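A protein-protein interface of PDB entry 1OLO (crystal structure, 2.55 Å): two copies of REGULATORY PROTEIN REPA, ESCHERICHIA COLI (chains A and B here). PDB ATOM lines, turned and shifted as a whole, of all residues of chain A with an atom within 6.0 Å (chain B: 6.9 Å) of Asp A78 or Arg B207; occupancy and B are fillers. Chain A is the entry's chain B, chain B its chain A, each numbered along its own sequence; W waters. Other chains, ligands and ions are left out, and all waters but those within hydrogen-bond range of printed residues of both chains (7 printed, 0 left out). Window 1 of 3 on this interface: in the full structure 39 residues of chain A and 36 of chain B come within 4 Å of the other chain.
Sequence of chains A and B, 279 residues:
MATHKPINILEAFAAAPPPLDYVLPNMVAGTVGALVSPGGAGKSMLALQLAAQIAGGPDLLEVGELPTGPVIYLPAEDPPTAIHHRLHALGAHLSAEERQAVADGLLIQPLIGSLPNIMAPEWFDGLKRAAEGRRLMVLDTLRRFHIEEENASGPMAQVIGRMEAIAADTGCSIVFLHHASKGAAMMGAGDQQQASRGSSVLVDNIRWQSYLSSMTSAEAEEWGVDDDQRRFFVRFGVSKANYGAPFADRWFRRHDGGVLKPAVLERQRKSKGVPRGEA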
ATOM      1  N   GLY A  40     -16.049  -6.978   6.022  1.00  0.00           N
ATOM      2  CA  GLY A  40     -15.772  -7.135   7.434  1.00  0.00           C
ATOM      3  C   GLY A  40     -16.687  -6.346   8.352  1.00  0.00           C
ATOM      4  O   GLY A  40     -16.599  -6.518   9.557  1.00  0.00           O
ATOM      5  N   SER A  44     -22.930 -10.000   6.307  1.00  0.00           N
ATOM      6  CA  SER A  44     -23.349 -11.405   6.353  1.00  0.00           C
ATOM      7  C   SER A  44     -24.121 -11.737   7.605  1.00  0.00           C
ATOM      8  O   SER A  44     -25.126 -12.442   7.518  1.00  0.00           O
ATOM      9  CB  SER A  44     -22.159 -12.352   6.255  1.00  0.00           C
ATOM     10  OG  SER A  44     -21.555 -12.304   4.966  1.00  0.00           O
ATOM     11  N   TYR A  73     -31.196 -17.790   1.444  1.00  0.00           N
ATOM     12  CA  TYR A  73     -29.955 -17.065   1.621  1.00  0.00           C
ATOM     13  C   TYR A  73     -28.896 -17.788   0.775  1.00  0.00           C
ATOM     14  O   TYR A  73     -28.733 -19.006   0.875  1.00  0.00           O
ATOM     15  CB  TYR A  73     -29.622 -16.882   3.117  1.00  0.00           C
ATOM     16  CG  TYR A  73     -28.216 -16.367   3.401  1.00  0.00           C
ATOM     17  CD1 TYR A  73     -27.697 -15.252   2.788  1.00  0.00           C
ATOM     18  CD2 TYR A  73     -27.391 -17.030   4.268  1.00  0.00           C
ATOM     19  CE1 TYR A  73     -26.406 -14.790   3.034  1.00  0.00           C
ATOM     20  CE2 TYR A  73     -26.106 -16.558   4.560  1.00  0.00           C
ATOM     21  CZ  TYR A  73     -25.595 -15.439   3.935  1.00  0.00           C
ATOM     22  OH  TYR A  73     -24.230 -15.019   4.245  1.00  0.00           O
ATOM     23  N   PRO A  75     -25.146 -17.625   0.423  1.00  0.00           N
ATOM     24  CA  PRO A  75     -23.782 -17.158   0.711  1.00  0.00           C
ATOM     25  C   PRO A  75     -22.760 -17.805  -0.283  1.00  0.00           C
ATOM     26  O   PRO A  75     -22.658 -19.046  -0.395  1.00  0.00           O
ATOM     27  CB  PRO A  75     -23.560 -17.647   2.125  1.00  0.00           C
ATOM     28  CG  PRO A  75     -24.396 -18.917   2.184  1.00  0.00           C
ATOM     29  CD  PRO A  75     -25.587 -18.709   1.321  1.00  0.00           C
ATOM     30  N   ALA A  76     -22.024 -16.984  -1.019  1.00  0.00           N
ATOM     31  CA  ALA A  76     -21.058 -17.522  -1.979  1.00  0.00           C
ATOM     32  C   ALA A  76     -19.599 -17.284  -1.574  1.00  0.00           C
ATOM     33  O   ALA A  76     -18.681 -17.608  -2.327  1.00  0.00           O
ATOM     34  CB  ALA A  76     -21.317 -16.940  -3.371  1.00  0.00           C
ATOM     35  N   GLU A  77     -19.387 -16.718  -0.394  1.00  0.00           N
ATOM     36  CA  GLU A  77     -18.077 -16.280   0.026  1.00  0.00           C
ATOM     37  C   GLU A  77     -17.596 -16.943   1.270  1.00  0.00           C
ATOM     38  O   GLU A  77     -16.417 -16.984   1.485  1.00  0.00           O
ATOM     39  CB  GLU A  77     -18.106 -14.796   0.285  1.00  0.00           C
ATOM     40  CG  GLU A  77     -18.298 -14.079  -0.997  1.00  0.00           C
ATOM     41  CD  GLU A  77     -18.192 -12.582  -0.905  1.00  0.00           C
ATOM     42  OE1 GLU A  77     -17.649 -12.049   0.122  1.00  0.00           O
ATOM     43  OE2 GLU A  77     -18.663 -11.988  -1.919  1.00  0.00           O
ATOM     44  N   ASP A  78     -18.504 -17.373   2.124  1.00  0.00           N
ATOM     45  CA  ASP A  78     -18.157 -18.115   3.348  1.00  0.00           C
ATOM     46  C   ASP A  78     -18.396 -19.596   3.230  1.00  0.00           C
ATOM     47  O   ASP A  78     -19.446 -20.039   2.750  1.00  0.00           O
ATOM     48  CB  ASP A  78     -18.991 -17.648   4.521  1.00  0.00           C
ATOM     49  CG  ASP A  78     -18.337 -16.530   5.237  1.00  0.00           C
ATOM     50  OD1 ASP A  78     -19.095 -15.570   5.574  1.00  0.00           O
ATOM     51  OD2 ASP A  78     -17.075 -16.527   5.454  1.00  0.00           O
ATOM     52  N   PRO A  79     -17.439 -20.363   3.722  1.00  0.00           N
ATOM     53  CA  PRO A  79     -17.587 -21.821   3.763  1.00  0.00           C
ATOM     54  C   PRO A  79     -18.718 -22.210   4.752  1.00  0.00           C
ATOM     55  O   PRO A  79     -18.940 -21.529   5.774  1.00  0.00           O
ATOM     56  CB  PRO A  79     -16.205 -22.284   4.292  1.00  0.00           C
ATOM     57  CG  PRO A  79     -15.675 -21.086   5.086  1.00  0.00           C
ATOM     58  CD  PRO A  79     -16.192 -19.878   4.359  1.00  0.00           C
ATOM     59  N   PRO A  80     -19.399 -23.310   4.469  1.00  0.00           N
ATOM     60  CA  PRO A  80     -20.418 -23.855   5.379  1.00  0.00           C
ATOM     61  C   PRO A  80     -20.100 -23.754   6.877  1.00  0.00           C
ATOM     62  O   PRO A  80     -20.979 -23.294   7.623  1.00  0.00           O
ATOM     63  CB  PRO A  80     -20.503 -25.330   4.956  1.00  0.00           C
ATOM     64  CG  PRO A  80     -20.298 -25.267   3.500  1.00  0.00           C
ATOM     65  CD  PRO A  80     -19.261 -24.143   3.261  1.00  0.00           C
ATOM     66  N   ALA A  82     -18.424 -21.754   8.591  1.00  0.00           N
ATOM     67  CA  ALA A  82     -18.576 -20.395   9.109  1.00  0.00           C
ATOM     68  C   ALA A  82     -20.095 -20.065   9.287  1.00  0.00           C
ATOM     69  O   ALA A  82     -20.522 -19.438  10.317  1.00  0.00           O
ATOM     70  CB  ALA A  82     -17.918 -19.421   8.178  1.00  0.00           C
ATOM     71  N   ILE A  83     -20.893 -20.517   8.308  1.00  0.00           N
ATOM     72  CA  ILE A  83     -22.298 -20.315   8.410  1.00  0.00           C
ATOM     73  C   ILE A  83     -22.819 -21.041   9.674  1.00  0.00           C
ATOM     74  O   ILE A  83     -23.640 -20.484  10.412  1.00  0.00           O
ATOM     75  CB  ILE A  83     -23.054 -20.807   7.133  1.00  0.00           C
ATOM     76  CG1 ILE A  83     -22.470 -20.268   5.811  1.00  0.00           C
ATOM     77  CG2 ILE A  83     -24.583 -20.606   7.290  1.00  0.00           C
ATOM     78  CD1 ILE A  83     -22.474 -18.825   5.694  1.00  0.00           C
ATOM     79  N   ARG A  86     -22.200 -18.929  12.808  1.00  0.00           N
ATOM     80  CA  ARG A  86     -23.041 -17.740  12.914  1.00  0.00           C
ATOM     81  C   ARG A  86     -24.401 -18.165  13.359  1.00  0.00           C
ATOM     82  O   ARG A  86     -24.985 -17.545  14.247  1.00  0.00           O
ATOM     83  CB  ARG A  86     -23.209 -17.065  11.577  1.00  0.00           C
ATOM     84  CG  ARG A  86     -21.959 -16.495  10.972  1.00  0.00           C
ATOM     85  CD  ARG A  86     -22.181 -15.242  10.015  1.00  0.00           C
ATOM     86  NE  ARG A  86     -20.838 -14.835   9.629  1.00  0.00           N
ATOM     87  CZ  ARG A  86     -20.261 -15.165   8.462  1.00  0.00           C
ATOM     88  NH1 ARG A  86     -21.001 -15.848   7.535  1.00  0.00           N
ATOM     89  NH2 ARG A  86     -18.957 -14.800   8.226  1.00  0.00           N
ATOM     90  N   PRO A 110     -25.275 -22.853   0.328  1.00  0.00           N
ATOM     91  CA  PRO A 110     -23.920 -22.329   0.140  1.00  0.00           C
ATOM     92  C   PRO A 110     -23.487 -22.500  -1.313  1.00  0.00           C
ATOM     93  O   PRO A 110     -23.797 -23.475  -1.968  1.00  0.00           O
ATOM     94  CB  PRO A 110     -23.062 -23.196   1.084  1.00  0.00           C
ATOM     95  CG  PRO A 110     -24.035 -23.806   2.063  1.00  0.00           C
ATOM     96  CD  PRO A 110     -25.275 -24.016   1.251  1.00  0.00           C
ATOM     97  N   LEU A 111     -22.768 -21.497  -1.797  1.00  0.00           N
ATOM     98  CA  LEU A 111     -22.343 -21.454  -3.180  1.00  0.00           C
ATOM     99  C   LEU A 111     -20.831 -21.185  -3.274  1.00  0.00           C
ATOM    100  O   LEU A 111     -20.332 -21.000  -4.372  1.00  0.00           O
ATOM    101  CB  LEU A 111     -23.155 -20.394  -3.986  1.00  0.00           C
ATOM    102  CG  LEU A 111     -24.602 -20.796  -4.349  1.00  0.00           C
ATOM    103  CD1 LEU A 111     -25.284 -19.696  -5.083  1.00  0.00           C
ATOM    104  CD2 LEU A 111     -24.667 -22.087  -5.200  1.00  0.00           C
ATOM    105  N   ILE A 112     -20.083 -21.187  -2.164  1.00  0.00           N
ATOM    106  CA  ILE A 112     -18.617 -20.938  -2.268  1.00  0.00           C
ATOM    107  C   ILE A 112     -17.953 -21.918  -3.273  1.00  0.00           C
ATOM    108  O   ILE A 112     -18.183 -23.153  -3.203  1.00  0.00           O
ATOM    109  CB  ILE A 112     -17.919 -20.977  -0.855  1.00  0.00           C
ATOM    110  CG1 ILE A 112     -16.520 -20.345  -0.917  1.00  0.00           C
ATOM    111  CG2 ILE A 112     -17.935 -22.396  -0.240  1.00  0.00           C
ATOM    112  CD1 ILE A 112     -15.830 -20.239   0.462  1.00  0.00           C
ATOM    113  N   ASP A 140     -25.026 -13.035  -1.361  1.00  0.00           N
ATOM    114  CA  ASP A 140     -23.943 -12.602  -0.470  1.00  0.00           C
ATOM    115  C   ASP A 140     -22.587 -13.049  -1.043  1.00  0.00           C
ATOM    116  O   ASP A 140     -22.233 -14.223  -0.870  1.00  0.00           O
ATOM    117  CB  ASP A 140     -24.228 -13.190   0.936  1.00  0.00           C
ATOM    118  CG  ASP A 140     -23.234 -12.732   2.020  1.00  0.00           C
ATOM    119  OD1 ASP A 140     -22.236 -12.035   1.722  1.00  0.00           O
ATOM    120  OD2 ASP A 140     -23.364 -13.064   3.231  1.00  0.00           O
ATOM    121  N   THR A 141     -21.844 -12.193  -1.758  1.00  0.00           N
ATOM    122  CA  THR A 141     -22.236 -10.855  -2.233  1.00  0.00           C
ATOM    123  C   THR A 141     -22.369 -10.874  -3.739  1.00  0.00           C
ATOM    124  O   THR A 141     -21.955 -11.836  -4.379  1.00  0.00           O
ATOM    125  CB  THR A 141     -21.163  -9.768  -1.880  1.00  0.00           C
ATOM    126  OG1 THR A 141     -19.993  -9.937  -2.706  1.00  0.00           O
ATOM    127  CG2 THR A 141     -20.662  -9.895  -0.393  1.00  0.00           C
ATOM    128  N   ARG A 144     -19.817 -12.235  -6.545  1.00  0.00           N
ATOM    129  CA  ARG A 144     -19.638 -13.656  -6.869  1.00  0.00           C
ATOM    130  C   ARG A 144     -20.703 -14.168  -7.831  1.00  0.00           C
ATOM    131  O   ARG A 144     -20.635 -15.359  -8.262  1.00  0.00           O
ATOM    132  CB  ARG A 144     -19.698 -14.530  -5.631  1.00  0.00           C
ATOM    133  CG  ARG A 144     -18.635 -14.187  -4.585  1.00  0.00           C
ATOM    134  CD  ARG A 144     -17.269 -14.190  -5.074  1.00  0.00           C
ATOM    135  NE  ARG A 144     -16.248 -14.379  -4.024  1.00  0.00           N
ATOM    136  CZ  ARG A 144     -15.661 -13.390  -3.285  1.00  0.00           C
ATOM    137  NH1 ARG A 144     -16.050 -12.088  -3.381  1.00  0.00           N
ATOM    138  NH2 ARG A 144     -14.686 -13.711  -2.441  1.00  0.00           N
ATOM    139  N   HIS A 179     -19.550  -5.400  -1.306  1.00  0.00           N
ATOM    140  CA  HIS A 179     -18.362  -4.859  -0.641  1.00  0.00           C
ATOM    141  C   HIS A 179     -17.952  -3.514  -1.306  1.00  0.00           C
ATOM    142  O   HIS A 179     -17.697  -3.489  -2.501  1.00  0.00           O
ATOM    143  CB  HIS A 179     -17.184  -5.861  -0.706  1.00  0.00           C
ATOM    144  CG  HIS A 179     -17.440  -7.188  -0.047  1.00  0.00           C
ATOM    145  ND1 HIS A 179     -17.986  -7.311   1.219  1.00  0.00           N
ATOM    146  CD2 HIS A 179     -17.177  -8.456  -0.468  1.00  0.00           C
ATOM    147  CE1 HIS A 179     -18.063  -8.595   1.543  1.00  0.00           C
ATOM    148  NE2 HIS A 179     -17.590  -9.311   0.530  1.00  0.00           N
ATOM    149  N   HIS B   4     -22.744 -27.992  -2.665  1.00  0.00           N
ATOM    150  CA  HIS B   4     -23.011 -28.036  -1.232  1.00  0.00           C
ATOM    151  C   HIS B   4     -24.386 -28.504  -0.908  1.00  0.00           C
ATOM    152  O   HIS B   4     -25.327 -28.158  -1.576  1.00  0.00           O
ATOM    153  CB  HIS B   4     -22.745 -26.674  -0.615  1.00  0.00           C
ATOM    154  CG  HIS B   4     -21.423 -26.096  -0.999  1.00  0.00           C
ATOM    155  ND1 HIS B   4     -20.254 -26.389  -0.316  1.00  0.00           N
ATOM    156  CD2 HIS B   4     -21.081 -25.261  -2.005  1.00  0.00           C
ATOM    157  CE1 HIS B   4     -19.252 -25.734  -0.880  1.00  0.00           C
ATOM    158  NE2 HIS B   4     -19.727 -25.050  -1.912  1.00  0.00           N
ATOM    159  N   ASN B  26      -6.967 -16.406  12.009  1.00  0.00           N
ATOM    160  CA  ASN B  26      -8.211 -15.792  11.494  1.00  0.00           C
ATOM    161  C   ASN B  26      -8.648 -16.133  10.049  1.00  0.00           C
ATOM    162  O   ASN B  26      -9.576 -15.516   9.504  1.00  0.00           O
ATOM    163  CB  ASN B  26      -8.117 -14.276  11.649  1.00  0.00           C
ATOM    164  CG  ASN B  26      -8.086 -13.852  13.102  1.00  0.00           C
ATOM    165  OD1 ASN B  26      -7.068 -13.364  13.607  1.00  0.00           O
ATOM    166  ND2 ASN B  26      -9.200 -14.058  13.788  1.00  0.00           N
ATOM    167  N   VAL B  28     -10.143 -19.071   7.875  1.00  0.00           N
ATOM    168  CA  VAL B  28     -10.784 -20.389   7.886  1.00  0.00           C
ATOM    169  C   VAL B  28     -10.201 -21.301   6.780  1.00  0.00           C
ATOM    170  O   VAL B  28      -9.962 -20.851   5.650  1.00  0.00           O
ATOM    171  CB  VAL B  28     -12.314 -20.224   7.716  1.00  0.00           C
ATOM    172  CG1 VAL B  28     -13.015 -21.581   7.622  1.00  0.00           C
ATOM    173  CG2 VAL B  28     -12.882 -19.377   8.855  1.00  0.00           C
ATOM    174  N   THR B  31     -10.433 -21.738   2.204  1.00  0.00           N
ATOM    175  CA  THR B  31     -10.779 -20.488   1.597  1.00  0.00           C
ATOM    176  C   THR B  31      -9.561 -19.867   0.966  1.00  0.00           C
ATOM    177  O   THR B  31      -8.499 -20.462   0.967  1.00  0.00           O
ATOM    178  CB  THR B  31     -11.395 -19.545   2.590  1.00  0.00           C
ATOM    179  OG1 THR B  31     -10.416 -19.202   3.582  1.00  0.00           O
ATOM    180  CG2 THR B  31     -12.544 -20.261   3.352  1.00  0.00           C
ATOM    181  N   VAL B  32      -9.771 -18.698   0.372  1.00  0.00           N
ATOM    182  CA  VAL B  32      -8.743 -17.962  -0.328  1.00  0.00           C
ATOM    183  C   VAL B  32      -8.412 -16.697   0.478  1.00  0.00           C
ATOM    184  O   VAL B  32      -9.303 -16.031   0.958  1.00  0.00           O
ATOM    185  CB  VAL B  32      -9.200 -17.644  -1.764  1.00  0.00           C
ATOM    186  CG1 VAL B  32      -8.133 -16.856  -2.527  1.00  0.00           C
ATOM    187  CG2 VAL B  32      -9.560 -18.949  -2.498  1.00  0.00           C
ATOM    188  N   GLY B  33      -7.134 -16.427   0.711  1.00  0.00           N
ATOM    189  CA  GLY B  33      -6.709 -15.219   1.424  1.00  0.00           C
ATOM    190  C   GLY B  33      -5.574 -14.522   0.700  1.00  0.00           C
ATOM    191  O   GLY B  33      -4.988 -15.065  -0.256  1.00  0.00           O
ATOM    192  N   ALA B  34      -5.244 -13.325   1.138  1.00  0.00           N
ATOM    193  CA  ALA B  34      -4.190 -12.564   0.442  1.00  0.00           C
ATOM    194  C   ALA B  34      -3.128 -12.102   1.393  1.00  0.00           C
ATOM    195  O   ALA B  34      -3.431 -11.702   2.541  1.00  0.00           O
ATOM    196  CB  ALA B  34      -4.781 -11.341  -0.235  1.00  0.00           C
ATOM    197  N   GLU B 164     -11.145 -19.982  -5.632  1.00  0.00           N
ATOM    198  CA  GLU B 164     -12.181 -20.370  -4.673  1.00  0.00           C
ATOM    199  C   GLU B 164     -12.747 -21.701  -5.026  1.00  0.00           C
ATOM    200  O   GLU B 164     -13.018 -22.478  -4.125  1.00  0.00           O
ATOM    201  CB  GLU B 164     -13.300 -19.341  -4.515  1.00  0.00           C
ATOM    202  CG  GLU B 164     -12.815 -18.062  -3.855  1.00  0.00           C
ATOM    203  CD  GLU B 164     -13.910 -17.020  -3.653  1.00  0.00           C
ATOM    204  OE1 GLU B 164     -13.691 -16.198  -2.755  1.00  0.00           O
ATOM    205  OE2 GLU B 164     -14.965 -16.997  -4.370  1.00  0.00           O
ATOM    206  N   VAL B 203      -8.401  -6.751  -3.434  1.00  0.00           N
ATOM    207  CA  VAL B 203      -8.475  -6.952  -2.008  1.00  0.00           C
ATOM    208  C   VAL B 203      -9.903  -6.767  -1.505  1.00  0.00           C
ATOM    209  O   VAL B 203     -10.303  -7.456  -0.558  1.00  0.00           O
ATOM    210  CB  VAL B 203      -7.402  -6.074  -1.214  1.00  0.00           C
ATOM    211  CG1 VAL B 203      -6.002  -6.052  -1.946  1.00  0.00           C
ATOM    212  CG2 VAL B 203      -7.927  -4.610  -0.801  1.00  0.00           C
ATOM    213  N   ASP B 204     -10.680  -5.884  -2.142  1.00  0.00           N
ATOM    214  CA  ASP B 204     -12.085  -5.685  -1.759  1.00  0.00           C
ATOM    215  C   ASP B 204     -12.989  -6.919  -1.625  1.00  0.00           C
ATOM    216  O   ASP B 204     -13.936  -6.895  -0.827  1.00  0.00           O
ATOM    217  CB  ASP B 204     -12.762  -4.630  -2.639  1.00  0.00           C
ATOM    218  CG  ASP B 204     -11.982  -3.315  -2.644  1.00  0.00           C
ATOM    219  OD1 ASP B 204     -12.143  -2.483  -3.579  1.00  0.00           O
ATOM    220  OD2 ASP B 204     -11.141  -3.057  -1.740  1.00  0.00           O
ATOM    221  N   ASN B 205     -12.698  -7.970  -2.379  1.00  0.00           N
ATOM    222  CA  ASN B 205     -13.515  -9.158  -2.406  1.00  0.00           C
ATOM    223  C   ASN B 205     -12.730 -10.430  -1.995  1.00  0.00           C
ATOM    224  O   ASN B 205     -13.066 -11.553  -2.391  1.00  0.00           O
ATOM    225  CB  ASN B 205     -14.134  -9.287  -3.800  1.00  0.00           C
ATOM    226  CG  ASN B 205     -15.180  -8.174  -4.090  1.00  0.00           C
ATOM    227  OD1 ASN B 205     -16.351  -8.226  -3.625  1.00  0.00           O
ATOM    228  ND2 ASN B 205     -14.748  -7.139  -4.826  1.00  0.00           N
ATOM    229  N   ILE B 206     -11.657 -10.259  -1.221  1.00  0.00           N
ATOM    230  CA  ILE B 206     -11.024 -11.389  -0.556  1.00  0.00           C
ATOM    231  C   ILE B 206     -11.422 -11.235   0.901  1.00  0.00           C
ATOM    232  O   ILE B 206     -11.440 -10.111   1.404  1.00  0.00           O
ATOM    233  CB  ILE B 206      -9.520 -11.352  -0.791  1.00  0.00           C
ATOM    234  CG1 ILE B 206      -9.272 -11.680  -2.249  1.00  0.00           C
ATOM    235  CG2 ILE B 206      -8.868 -12.478  -0.116  1.00  0.00           C
ATOM    236  CD1 ILE B 206      -9.970 -13.018  -2.750  1.00  0.00           C
ATOM    237  N   ARG B 207     -11.815 -12.325   1.546  1.00  0.00           N
ATOM    238  CA  ARG B 207     -12.315 -12.243   2.914  1.00  0.00           C
ATOM    239  C   ARG B 207     -11.229 -12.183   4.030  1.00  0.00           C
ATOM    240  O   ARG B 207     -11.505 -11.673   5.110  1.00  0.00           O
ATOM    241  CB  ARG B 207     -13.333 -13.368   3.161  1.00  0.00           C
ATOM    242  CG  ARG B 207     -14.725 -13.062   2.588  1.00  0.00           C
ATOM    243  CD  ARG B 207     -15.831 -13.894   3.194  1.00  0.00           C
ATOM    244  NE  ARG B 207     -16.602 -13.283   4.283  1.00  0.00           N
ATOM    245  CZ  ARG B 207     -17.586 -12.371   4.163  1.00  0.00           C
ATOM    246  NH1 ARG B 207     -17.986 -11.883   2.974  1.00  0.00           N
ATOM    247  NH2 ARG B 207     -18.215 -11.982   5.271  1.00  0.00           N
ATOM    248  N   TRP B 208     -10.021 -12.706   3.772  1.00  0.00           N
ATOM    249  CA  TRP B 208      -8.867 -12.604   4.682  1.00  0.00           C
ATOM    250  C   TRP B 208      -7.713 -11.912   3.994  1.00  0.00           C
ATOM    251  O   TRP B 208      -7.314 -12.282   2.894  1.00  0.00           O
ATOM    252  CB  TRP B 208      -8.391 -13.975   5.073  1.00  0.00           C
ATOM    253  CG  TRP B 208      -7.345 -14.026   6.146  1.00  0.00           C
ATOM    254  CD1 TRP B 208      -7.567 -14.035   7.513  1.00  0.00           C
ATOM    255  CD2 TRP B 208      -5.916 -14.150   5.974  1.00  0.00           C
ATOM    256  NE1 TRP B 208      -6.376 -14.149   8.178  1.00  0.00           N
ATOM    257  CE2 TRP B 208      -5.347 -14.241   7.270  1.00  0.00           C
ATOM    258  CE3 TRP B 208      -5.055 -14.211   4.852  1.00  0.00           C
ATOM    259  CZ2 TRP B 208      -3.958 -14.345   7.481  1.00  0.00           C
ATOM    260  CZ3 TRP B 208      -3.657 -14.327   5.065  1.00  0.00           C
ATOM    261  CH2 TRP B 208      -3.134 -14.410   6.365  1.00  0.00           C
ATOM    262  N   GLN B 209      -7.145 -10.932   4.666  1.00  0.00           N
ATOM    263  CA  GLN B 209      -6.084 -10.111   4.106  1.00  0.00           C
ATOM    264  C   GLN B 209      -5.041  -9.845   5.178  1.00  0.00           C
ATOM    265  O   GLN B 209      -5.357  -9.297   6.225  1.00  0.00           O
ATOM    266  CB  GLN B 209      -6.679  -8.795   3.653  1.00  0.00           C
ATOM    267  CG  GLN B 209      -6.026  -8.249   2.412  1.00  0.00           C
ATOM    268  CD  GLN B 209      -5.395  -6.823   2.604  1.00  0.00           C
ATOM    269  OE1 GLN B 209      -4.269  -6.656   3.142  1.00  0.00           O
ATOM    270  NE2 GLN B 209      -6.116  -5.825   2.161  1.00  0.00           N
ATOM    271  N   LYS B 240      -7.833  -7.615   7.331  1.00  0.00           N
ATOM    272  CA  LYS B 240      -9.241  -7.986   7.163  1.00  0.00           C
ATOM    273  C   LYS B 240      -9.461  -9.457   7.483  1.00  0.00           C
ATOM    274  O   LYS B 240      -8.676 -10.312   7.044  1.00  0.00           O
ATOM    275  CB  LYS B 240      -9.673  -7.680   5.727  1.00  0.00           C
ATOM    276  CG  LYS B 240     -11.148  -7.819   5.467  1.00  0.00           C
ATOM    277  CD  LYS B 240     -11.550  -7.107   4.159  1.00  0.00           C
ATOM    278  CE  LYS B 240     -10.706  -7.523   2.962  1.00  0.00           C
ATOM    279  NZ  LYS B 240     -11.592  -7.513   1.804  1.00  0.00           N
ATOM    280  N   ALA B 241     -10.513  -9.749   8.255  1.00  0.00           N
ATOM    281  CA  ALA B 241     -10.930 -11.134   8.496  1.00  0.00           C
ATOM    282  C   ALA B 241     -12.365 -11.125   9.018  1.00  0.00           C
ATOM    283  O   ALA B 241     -12.867 -10.086   9.455  1.00  0.00           O
ATOM    284  CB  ALA B 241      -9.979 -11.865   9.478  1.00  0.00           C
ATOM    285  N   ASN B 242     -13.057 -12.261   8.953  1.00  0.00           N
ATOM    286  CA  ASN B 242     -14.416 -12.261   9.493  1.00  0.00           C
ATOM    287  C   ASN B 242     -14.350 -12.413  11.007  1.00  0.00           C
ATOM    288  O   ASN B 242     -13.299 -12.829  11.529  1.00  0.00           O
ATOM    289  CB  ASN B 242     -15.410 -13.221   8.767  1.00  0.00           C
ATOM    290  CG  ASN B 242     -15.102 -14.708   8.955  1.00  0.00           C
ATOM    291  OD1 ASN B 242     -14.780 -15.166  10.060  1.00  0.00           O
ATOM    292  ND2 ASN B 242     -15.277 -15.483   7.877  1.00  0.00           N
HETATM  293  O   HOH W   1     -17.024 -18.512  -4.358  1.00  0.00           O
HETATM  294  O   HOH W   2     -20.430 -10.422   3.093  1.00  0.00           O
HETATM  295  O   HOH W   3     -19.016  -7.534  -3.326  1.00  0.00           O
HETATM  296  O   HOH W   4     -14.942 -11.662  -0.381  1.00  0.00           O
HETATM  297  O   HOH W   5     -17.474  -5.608  -5.266  1.00  0.00           O
HETATM  298  O   HOH W   6     -14.331  -8.867   1.486  1.00  0.00           O
HETATM  299  O   HOH W   7     -17.377 -14.903  10.865  1.00  0.00           O
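O of Ile A112 sits at hydrogen-bond distance from NE2 of His B4 (2.8 Å). The guanidinium group (NH2) of Arg A144 is in salt-bridge range of the side-chain carboxylate (OE1) of Glu B164 (2.7 Å). The backbone carbonyl oxygen of Asn B205 lies within hydrogen-bond range of the guanidinium group of Arg A144. The guanidinium group of Arg B207 lies within hydrogen-bond range of the side-chain hydroxyl of Ser A44 (3.4 Å). NH1 of Arg B207 is in salt-bridge range of OE1 of Glu A77 (2.9 Å). OD2 of Asp A78 lies within salt-bridge range of NE of Arg B207, at 3.5 Å. The side-chain carboxylate (OD2) of Asp A78 lies within hydrogen-bond range of the side-chain amide nitrogen (ND2) of Asn B242, at 3.2 Å.
The backbone carbonyl oxygen (O) of Val B28 is in hydrogen-bond range of the side-chain hydroxyl (OG1) of Thr B31. OG of Ser A44 is in hydrogen-bond range of OD2 of Asp A140, at 2.6 Å. OG1 of Thr A141 is in hydrogen-bond range of OE2 of Glu A77 (2.6 Å). OE2 of Glu A77 lies within salt-bridge range of NH1 of Arg A144 (3.0 Å). The side-chain carboxylate (OE1) of Glu A77 sits at hydrogen-bond distance from a ring nitrogen (NE2) of His A179, 2.8 Å away. The guanidinium group (NH1) of Arg A86 is in salt-bridge range of the side-chain carboxylate (OD1) of Asp A78.
Among the printed residues, pairs that only touch across the chains: Pro A110 with His B4 (3.3 Å), His A179 with Asn B205 (3.3 Å), His A179 with Asp B204 (3.4 Å), His A179 with Arg B207 (3.6 Å), Pro A79 with Thr B31 (3.7 Å), Pro A79 with Val B28 (3.7 Å), Arg A86 with Asn B242 (3.8 Å) and Pro A80 with His B4 (3.98 Å).
Printed residues of chain B within 4 Å of Asp A78: Arg B207 (3.5 Å) and Asn B242 (3.2 Å). Printed residues of chain A within 4 Å of Arg B207: Ser A44, Glu A77, Asp A78 and His A179. Of the printed residues of chain A, Asn B242 touches Asp A78 (3.2 Å) and Arg A86 (3.8 Å). Of the printed residues of chain B, Glu A77 touches Arg B207. Of the printed residues of chain B, Pro A80 touches His B4. Printed residues of chain B within 4 Å of Ser A44: Arg B207. Leu A111 touches none of the printed residues of chain B. The nearest residue of chain A that does not touch Arg B207 is Arg A86 (4.2 Å). The nearest printed residue of chain B that does not touch Pro A79 is Asn B242 (5.7 Å).
Of the 18 printed residues of chain B, 8 touch a printed residue of chain A. Printed residues of chain A that touch a printed residue of chain B: Ser A44, Glu A77, Asp A78, Pro A79, Pro A80, Arg A86, Pro A110, Ile A112, Arg A144 and His A179. Among the printed residues, 15 pairs touch across the chains.
No position is printed for both chains. Of the 15 pairs that touch across the chains among the printed residues, none has its exchanged pair printed and touching as well.
Water W1 lies within hydrogen-bond range of OE2 of Glu B164 (2.6 Å) and O of Ala A76 (2.8 Å). Water W4 lies within hydrogen-bond range of O of Asn B205 (2.8 Å), OE1 of Glu A77 (2.8 Å) and NH2 of Arg A144 (2.9 Å). Water W2 lies within hydrogen-bond range of the side-chain carboxylate (OD1) of Asp A140, the guanidinium group (NH1) of Arg B207 and the side-chain hydroxyl (OG) of Ser A44.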
